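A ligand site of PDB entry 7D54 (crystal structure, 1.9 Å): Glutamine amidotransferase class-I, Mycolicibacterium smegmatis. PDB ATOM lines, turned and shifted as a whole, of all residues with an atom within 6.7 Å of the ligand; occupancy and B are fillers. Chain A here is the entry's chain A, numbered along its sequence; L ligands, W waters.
OD2 of OCS 101 lies close to an oxygen (O3) of the ligand (2.4 Å).
O of Trp 144 sits close to O3 of the ligand (2.6 Å).
O of Ala 66 sits close to O1 of the ligand (2.7 Å).
The backbone carbonyl oxygen (O) of Trp 144 sits close to OD1 of OCS 101 (3.1 Å).
A ring nitrogen (NE2) of His 179 lies within hydrogen-bond range of OD1 of OCS 101 (2.5 Å).
OD3 of OCS 101 is in hydrogen-bond range of the side-chain amide nitrogen of Gln 177, at 2.9 Å.
The indole nitrogen (NE1) of Trp 190 lies within hydrogen-bond range of the backbone carbonyl oxygen (O) of Met 15 (2.9 Å).
The backbone carbonyl oxygen (O) of Phe 142 is in hydrogen-bond range of the backbone NH (N) of His 179.
The side-chain carboxylate (OE2) of Glu 181 lies within hydrogen-bond range of a ring nitrogen (ND1) of His 179 (2.8 Å).
Water W2 lies within hydrogen-bond range of O1 of the ligand (2.5 Å), O of Trp 68 (2.5 Å) and O of Ala 66 (3.0 Å).
Water W1 lies within hydrogen-bond range of O1 of the ligand (2.7 Å), OE1 of Gln 105 (2.8 Å) and OD3 of OCS 101 (2.9 Å).
Residues that only touch the ligand: Trp 190 (3.1 Å), Phe 146 (3.7 Å) and His 179 (3.7 Å).
Hydrophobic or aromatic side chains that line the ligand: Trp 144, Phe 146, His 179 and Trp 190.
Within 4 Å of the ligand: Ala 66, OCS 101, Trp 144, Phe 146, His 179 and Trp 190.
The nearest printed residue that does not touch the ligand is Arg 67 (4.02 Å).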
ATOM      1  N   GLU A  13      25.159  18.737   2.019  1.00  0.00           N
ATOM      2  CA  GLU A  13      26.056  19.109   3.108  1.00  0.00           C
ATOM      3  C   GLU A  13      25.244  19.791   4.195  1.00  0.00           C
ATOM      4  O   GLU A  13      24.248  20.483   3.912  1.00  0.00           O
ATOM      5  CB  GLU A  13      27.175  20.018   2.602  1.00  0.00           C
ATOM      6  CG  GLU A  13      28.104  20.495   3.665  1.00  0.00           C
ATOM      7  CD  GLU A  13      28.878  21.726   3.208  1.00  0.00           C
ATOM      8  OE1 GLU A  13      29.233  21.803   2.031  1.00  0.00           O
ATOM      9  OE2 GLU A  13      29.146  22.599   4.056  1.00  0.00           O
ATOM     10  N   MET A  15      25.548  22.219   6.298  1.00  0.00           N
ATOM     11  CA  MET A  15      25.368  23.651   6.435  1.00  0.00           C
ATOM     12  C   MET A  15      24.635  24.271   5.249  1.00  0.00           C
ATOM     13  O   MET A  15      24.472  25.487   5.216  1.00  0.00           O
ATOM     14  CB  MET A  15      26.721  24.347   6.593  1.00  0.00           C
ATOM     15  CG  MET A  15      27.476  24.118   7.908  1.00  0.00           C
ATOM     16  SD  MET A  15      26.469  23.674   9.341  1.00  0.00           S
ATOM     17  CE  MET A  15      25.416  25.084   9.562  1.00  0.00           C
ATOM     18  N   CYS A  16      24.242  23.475   4.261  1.00  0.00           N
ATOM     19  CA  CYS A  16      23.579  23.969   3.061  1.00  0.00           C
ATOM     20  C   CYS A  16      22.130  23.489   3.050  1.00  0.00           C
ATOM     21  O   CYS A  16      21.728  22.602   2.296  1.00  0.00           O
ATOM     22  CB  CYS A  16      24.354  23.510   1.798  1.00  0.00           C
ATOM     23  SG  CYS A  16      25.931  24.437   1.479  1.00  0.00           S
ATOM     24  N   GLY A  65      23.148  22.609  -2.103  1.00  0.00           N
ATOM     25  CA  GLY A  65      24.531  22.837  -2.433  1.00  0.00           C
ATOM     26  C   GLY A  65      25.487  22.069  -1.520  1.00  0.00           C
ATOM     27  O   GLY A  65      25.101  21.411  -0.558  1.00  0.00           O
ATOM     28  N   ALA A  66      26.779  22.152  -1.856  1.00  0.00           N
ATOM     29  CA  ALA A  66      27.809  21.521  -1.042  1.00  0.00           C
ATOM     30  C   ALA A  66      29.158  22.002  -1.555  1.00  0.00           C
ATOM     31  O   ALA A  66      29.264  22.562  -2.658  1.00  0.00           O
ATOM     32  CB  ALA A  66      27.756  19.987  -1.114  1.00  0.00           C
ATOM     33  N   ARG A  67      30.179  21.779  -0.734  1.00  0.00           N
ATOM     34  CA  ARG A  67      31.497  22.335  -1.040  1.00  0.00           C
ATOM     35  C   ARG A  67      32.379  21.432  -1.882  1.00  0.00           C
ATOM     36  O   ARG A  67      33.430  21.888  -2.348  1.00  0.00           O
ATOM     37  CB  ARG A  67      32.258  22.647   0.257  1.00  0.00           C
ATOM     38  CG  ARG A  67      32.537  21.379   1.024  1.00  0.00           C
ATOM     39  CD  ARG A  67      33.237  21.667   2.357  1.00  0.00           C
ATOM     40  NE  ARG A  67      32.292  22.164   3.346  1.00  0.00           N
ATOM     41  CZ  ARG A  67      32.629  22.631   4.538  1.00  0.00           C
ATOM     42  NH1 ARG A  67      33.900  22.643   4.917  1.00  0.00           N
ATOM     43  NH2 ARG A  67      31.681  23.047   5.367  1.00  0.00           N
ATOM     44  N   TRP A  68      32.030  20.173  -2.052  1.00  0.00           N
ATOM     45  CA  TRP A  68      32.945  19.279  -2.756  1.00  0.00           C
ATOM     46  C   TRP A  68      32.700  19.318  -4.266  1.00  0.00           C
ATOM     47  O   TRP A  68      31.638  19.757  -4.724  1.00  0.00           O
ATOM     48  CB  TRP A  68      32.795  17.848  -2.234  1.00  0.00           C
ATOM     49  CG  TRP A  68      32.669  17.804  -0.714  1.00  0.00           C
ATOM     50  CD1 TRP A  68      33.657  17.997   0.211  1.00  0.00           C
ATOM     51  CD2 TRP A  68      31.471  17.583   0.019  1.00  0.00           C
ATOM     52  NE1 TRP A  68      33.154  17.873   1.487  1.00  0.00           N
ATOM     53  CE2 TRP A  68      31.803  17.645   1.398  1.00  0.00           C
ATOM     54  CE3 TRP A  68      30.147  17.343  -0.353  1.00  0.00           C
ATOM     55  CZ2 TRP A  68      30.863  17.464   2.395  1.00  0.00           C
ATOM     56  CZ3 TRP A  68      29.211  17.144   0.648  1.00  0.00           C
ATOM     57  CH2 TRP A  68      29.573  17.225   1.997  1.00  0.00           C
ATOM     58  N   PRO A  69      33.679  18.884  -5.065  1.00  0.00           N
ATOM     59  CA  PRO A  69      33.442  18.812  -6.520  1.00  0.00           C
ATOM     60  C   PRO A  69      32.535  17.631  -6.831  1.00  0.00           C
ATOM     61  O   PRO A  69      32.811  16.493  -6.433  1.00  0.00           O
ATOM     62  CB  PRO A  69      34.838  18.629  -7.134  1.00  0.00           C
ATOM     63  CG  PRO A  69      35.836  18.685  -5.961  1.00  0.00           C
ATOM     64  CD  PRO A  69      35.043  18.447  -4.711  1.00  0.00           C
ATOM     65  N   OCS A 101      23.031  24.971  -7.058  1.00  0.00           N
ATOM     66  CA  OCS A 101      24.491  25.020  -7.017  1.00  0.00           C
ATOM     67  CB  OCS A 101      24.879  25.659  -5.717  1.00  0.00           C
ATOM     68  SG  OCS A 101      26.624  25.966  -5.443  1.00  0.00           S
ATOM     69  C   OCS A 101      25.035  23.626  -7.244  1.00  0.00           C
ATOM     70  O   OCS A 101      24.845  23.138  -8.335  1.00  0.00           O
ATOM     71  OD1 OCS A 101      26.872  27.280  -5.053  1.00  0.00           O
ATOM     72  OD2 OCS A 101      26.912  25.025  -4.328  1.00  0.00           O
ATOM     73  OD3 OCS A 101      27.414  25.638  -6.566  1.00  0.00           O
ATOM     74  N   PHE A 102      25.743  23.010  -6.281  1.00  0.00           N
ATOM     75  CA  PHE A 102      26.173  21.601  -6.391  1.00  0.00           C
ATOM     76  C   PHE A 102      25.013  20.715  -6.931  1.00  0.00           C
ATOM     77  O   PHE A 102      25.198  19.836  -7.773  1.00  0.00           O
ATOM     78  CB  PHE A 102      26.659  21.106  -5.014  1.00  0.00           C
ATOM     79  CG  PHE A 102      27.078  19.666  -4.984  1.00  0.00           C
ATOM     80  CD1 PHE A 102      26.146  18.679  -4.688  1.00  0.00           C
ATOM     81  CD2 PHE A 102      28.418  19.306  -5.157  1.00  0.00           C
ATOM     82  CE1 PHE A 102      26.522  17.366  -4.619  1.00  0.00           C
ATOM     83  CE2 PHE A 102      28.819  18.003  -5.066  1.00  0.00           C
ATOM     84  CZ  PHE A 102      27.887  17.002  -4.829  1.00  0.00           C
ATOM     85  N   GLN A 105      24.642  21.432 -10.561  1.00  0.00           N
ATOM     86  CA  GLN A 105      25.762  20.754 -11.224  1.00  0.00           C
ATOM     87  C   GLN A 105      25.535  19.245 -11.268  1.00  0.00           C
ATOM     88  O   GLN A 105      25.814  18.603 -12.288  1.00  0.00           O
ATOM     89  CB  GLN A 105      27.058  21.094 -10.546  1.00  0.00           C
ATOM     90  CG  GLN A 105      27.481  22.587 -10.723  1.00  0.00           C
ATOM     91  CD  GLN A 105      28.626  22.956  -9.798  1.00  0.00           C
ATOM     92  OE1 GLN A 105      29.041  22.150  -8.958  1.00  0.00           O
ATOM     93  NE2 GLN A 105      29.183  24.164  -9.965  1.00  0.00           N
ATOM     94  N   PHE A 142      22.554  35.454  -5.080  1.00  0.00           N
ATOM     95  CA  PHE A 142      23.806  35.185  -4.375  1.00  0.00           C
ATOM     96  C   PHE A 142      24.507  33.991  -4.981  1.00  0.00           C
ATOM     97  O   PHE A 142      23.882  32.944  -5.221  1.00  0.00           O
ATOM     98  CB  PHE A 142      23.577  34.931  -2.901  1.00  0.00           C
ATOM     99  CG  PHE A 142      24.864  34.797  -2.137  1.00  0.00           C
ATOM    100  CD1 PHE A 142      25.600  35.920  -1.759  1.00  0.00           C
ATOM    101  CD2 PHE A 142      25.362  33.551  -1.844  1.00  0.00           C
ATOM    102  CE1 PHE A 142      26.795  35.771  -1.069  1.00  0.00           C
ATOM    103  CE2 PHE A 142      26.516  33.406  -1.152  1.00  0.00           C
ATOM    104  CZ  PHE A 142      27.255  34.524  -0.793  1.00  0.00           C
ATOM    105  N   GLN A 143      25.812  34.130  -5.181  1.00  0.00           N
ATOM    106  CA  GLN A 143      26.649  33.103  -5.767  1.00  0.00           C
ATOM    107  C   GLN A 143      27.789  32.786  -4.824  1.00  0.00           C
ATOM    108  O   GLN A 143      28.347  33.676  -4.179  1.00  0.00           O
ATOM    109  CB  GLN A 143      27.265  33.573  -7.086  1.00  0.00           C
ATOM    110  CG  GLN A 143      26.273  34.128  -8.075  1.00  0.00           C
ATOM    111  CD  GLN A 143      25.919  33.083  -9.087  1.00  0.00           C
ATOM    112  OE1 GLN A 143      26.314  31.925  -8.954  1.00  0.00           O
ATOM    113  NE2 GLN A 143      25.164  33.483 -10.127  1.00  0.00           N
ATOM    114  N   TRP A 144      28.202  31.519  -4.810  1.00  0.00           N
ATOM    115  CA  TRP A 144      29.433  31.132  -4.137  1.00  0.00           C
ATOM    116  C   TRP A 144      29.860  29.809  -4.803  1.00  0.00           C
ATOM    117  O   TRP A 144      29.486  28.728  -4.341  1.00  0.00           O
ATOM    118  CB  TRP A 144      29.250  30.986  -2.647  1.00  0.00           C
ATOM    119  CG  TRP A 144      30.501  30.969  -1.892  1.00  0.00           C
ATOM    120  CD1 TRP A 144      31.715  30.481  -2.319  1.00  0.00           C
ATOM    121  CD2 TRP A 144      30.713  31.449  -0.547  1.00  0.00           C
ATOM    122  NE1 TRP A 144      32.640  30.638  -1.324  1.00  0.00           N
ATOM    123  CE2 TRP A 144      32.058  31.209  -0.227  1.00  0.00           C
ATOM    124  CE3 TRP A 144      29.877  32.032   0.411  1.00  0.00           C
ATOM    125  CZ2 TRP A 144      32.612  31.560   1.005  1.00  0.00           C
ATOM    126  CZ3 TRP A 144      30.443  32.361   1.671  1.00  0.00           C
ATOM    127  CH2 TRP A 144      31.790  32.140   1.936  1.00  0.00           C
ATOM    128  N   HIS A 145      30.631  29.915  -5.885  1.00  0.00           N
ATOM    129  CA  HIS A 145      31.011  28.681  -6.578  1.00  0.00           C
ATOM    130  C   HIS A 145      32.297  28.862  -7.371  1.00  0.00           C
ATOM    131  O   HIS A 145      32.586  29.944  -7.889  1.00  0.00           O
ATOM    132  CB  HIS A 145      29.876  28.169  -7.493  1.00  0.00           C
ATOM    133  CG  HIS A 145      29.702  28.961  -8.754  1.00  0.00           C
ATOM    134  ND1 HIS A 145      30.217  28.570  -9.962  1.00  0.00           N
ATOM    135  CD2 HIS A 145      29.021  30.114  -8.986  1.00  0.00           C
ATOM    136  CE1 HIS A 145      29.914  29.472 -10.885  1.00  0.00           C
ATOM    137  NE2 HIS A 145      29.181  30.410 -10.315  1.00  0.00           N
ATOM    138  N   PHE A 146      33.062  27.757  -7.486  1.00  0.00           N
ATOM    139  CA  PHE A 146      34.297  27.743  -8.268  1.00  0.00           C
ATOM    140  C   PHE A 146      34.311  26.744  -9.424  1.00  0.00           C
ATOM    141  O   PHE A 146      35.308  26.706 -10.158  1.00  0.00           O
ATOM    142  CB  PHE A 146      35.466  27.439  -7.332  1.00  0.00           C
ATOM    143  CG  PHE A 146      35.483  28.312  -6.114  1.00  0.00           C
ATOM    144  CD1 PHE A 146      36.077  29.566  -6.160  1.00  0.00           C
ATOM    145  CD2 PHE A 146      34.906  27.887  -4.942  1.00  0.00           C
ATOM    146  CE1 PHE A 146      36.087  30.376  -5.023  1.00  0.00           C
ATOM    147  CE2 PHE A 146      34.909  28.683  -3.813  1.00  0.00           C
ATOM    148  CZ  PHE A 146      35.494  29.935  -3.861  1.00  0.00           C
ATOM    149  N   ASP A 147      33.245  25.966  -9.588  1.00  0.00           N
ATOM    150  CA  ASP A 147      32.987  25.038 -10.671  1.00  0.00           C
ATOM    151  C   ASP A 147      31.826  25.576 -11.508  1.00  0.00           C
ATOM    152  O   ASP A 147      30.994  26.359 -11.026  1.00  0.00           O
ATOM    153  CB  ASP A 147      32.623  23.641 -10.141  1.00  0.00           C
ATOM    154  CG  ASP A 147      33.777  22.947  -9.469  1.00  0.00           C
ATOM    155  OD1 ASP A 147      34.915  23.068  -9.963  1.00  0.00           O
ATOM    156  OD2 ASP A 147      33.555  22.290  -8.417  1.00  0.00           O
ATOM    157  N   GLN A 177      22.650  27.629 -10.743  1.00  0.00           N
ATOM    158  CA  GLN A 177      24.015  27.708 -10.247  1.00  0.00           C
ATOM    159  C   GLN A 177      24.131  28.600  -9.026  1.00  0.00           C
ATOM    160  O   GLN A 177      25.107  28.462  -8.251  1.00  0.00           O
ATOM    161  CB  GLN A 177      24.917  28.182 -11.384  1.00  0.00           C
ATOM    162  CG  GLN A 177      26.401  28.279 -11.037  1.00  0.00           C
ATOM    163  CD  GLN A 177      27.002  26.974 -10.549  1.00  0.00           C
ATOM    164  OE1 GLN A 177      27.446  26.157 -11.339  1.00  0.00           O
ATOM    165  NE2 GLN A 177      27.017  26.779  -9.243  1.00  0.00           N
ATOM    166  N   HIS A 179      22.303  30.593  -5.424  1.00  0.00           N
ATOM    167  CA  HIS A 179      21.617  30.213  -4.198  1.00  0.00           C
ATOM    168  C   HIS A 179      20.436  31.122  -3.956  1.00  0.00           C
ATOM    169  O   HIS A 179      20.579  32.156  -3.299  1.00  0.00           O
ATOM    170  CB  HIS A 179      22.554  30.295  -2.999  1.00  0.00           C
ATOM    171  CG  HIS A 179      23.625  29.271  -2.976  1.00  0.00           C
ATOM    172  ND1 HIS A 179      23.484  28.038  -2.381  1.00  0.00           N
ATOM    173  CD2 HIS A 179      24.902  29.345  -3.427  1.00  0.00           C
ATOM    174  CE1 HIS A 179      24.624  27.382  -2.495  1.00  0.00           C
ATOM    175  NE2 HIS A 179      25.479  28.129  -3.158  1.00  0.00           N
ATOM    176  N   GLU A 181      18.124  30.747  -2.024  1.00  0.00           N
ATOM    177  CA  GLU A 181      17.592  30.494  -0.695  1.00  0.00           C
ATOM    178  C   GLU A 181      18.293  31.288   0.388  1.00  0.00           C
ATOM    179  O   GLU A 181      17.891  31.198   1.550  1.00  0.00           O
ATOM    180  CB  GLU A 181      17.669  28.994  -0.379  1.00  0.00           C
ATOM    181  CG  GLU A 181      19.066  28.449   0.065  1.00  0.00           C
ATOM    182  CD  GLU A 181      20.057  28.213  -1.095  1.00  0.00           C
ATOM    183  OE1 GLU A 181      19.738  28.574  -2.249  1.00  0.00           O
ATOM    184  OE2 GLU A 181      21.166  27.665  -0.823  1.00  0.00           O
ATOM    185  N   TRP A 190      27.791  29.905   6.744  1.00  0.00           N
ATOM    186  CA  TRP A 190      28.878  29.768   5.788  1.00  0.00           C
ATOM    187  C   TRP A 190      30.059  30.651   6.167  1.00  0.00           C
ATOM    188  O   TRP A 190      31.208  30.215   6.090  1.00  0.00           O
ATOM    189  CB  TRP A 190      28.380  30.141   4.393  1.00  0.00           C
ATOM    190  CG  TRP A 190      27.280  29.280   3.909  1.00  0.00           C
ATOM    191  CD1 TRP A 190      26.883  28.082   4.422  1.00  0.00           C
ATOM    192  CD2 TRP A 190      26.447  29.526   2.773  1.00  0.00           C
ATOM    193  NE1 TRP A 190      25.826  27.578   3.695  1.00  0.00           N
ATOM    194  CE2 TRP A 190      25.546  28.439   2.671  1.00  0.00           C
ATOM    195  CE3 TRP A 190      26.360  30.573   1.846  1.00  0.00           C
ATOM    196  CZ2 TRP A 190      24.573  28.356   1.673  1.00  0.00           C
ATOM    197  CZ3 TRP A 190      25.396  30.495   0.860  1.00  0.00           C
ATOM    198  CH2 TRP A 190      24.503  29.397   0.792  1.00  0.00           C
HETATM  199  N1  LIG L   1      32.134  26.512  -2.756  1.00  0.00           N
HETATM  200  C1  LIG L   1      30.802  26.032  -2.468  1.00  0.00           C
HETATM  201  C2  LIG L   1      30.023  25.511  -3.662  1.00  0.00           C
HETATM  202  O1  LIG L   1      30.317  24.464  -4.243  1.00  0.00           O
HETATM  203  C3  LIG L   1      30.000  27.158  -1.845  1.00  0.00           C
HETATM  204  C4  LIG L   1      28.680  26.748  -1.280  1.00  0.00           C
HETATM  205  C5  LIG L   1      28.386  27.494   0.006  1.00  0.00           C
HETATM  206  O2  LIG L   1      28.942  27.194   1.054  1.00  0.00           O
HETATM  207  N2  LIG L   1      27.535  28.500  -0.090  1.00  0.00           N
HETATM  208  O3  LIG L   1      29.054  26.149  -4.063  1.00  0.00           O
HETATM  209  O   HOH W   1      29.371  23.433  -6.508  1.00  0.00           O
HETATM  210  O   HOH W   2      31.118  22.228  -4.955  1.00  0.00           O
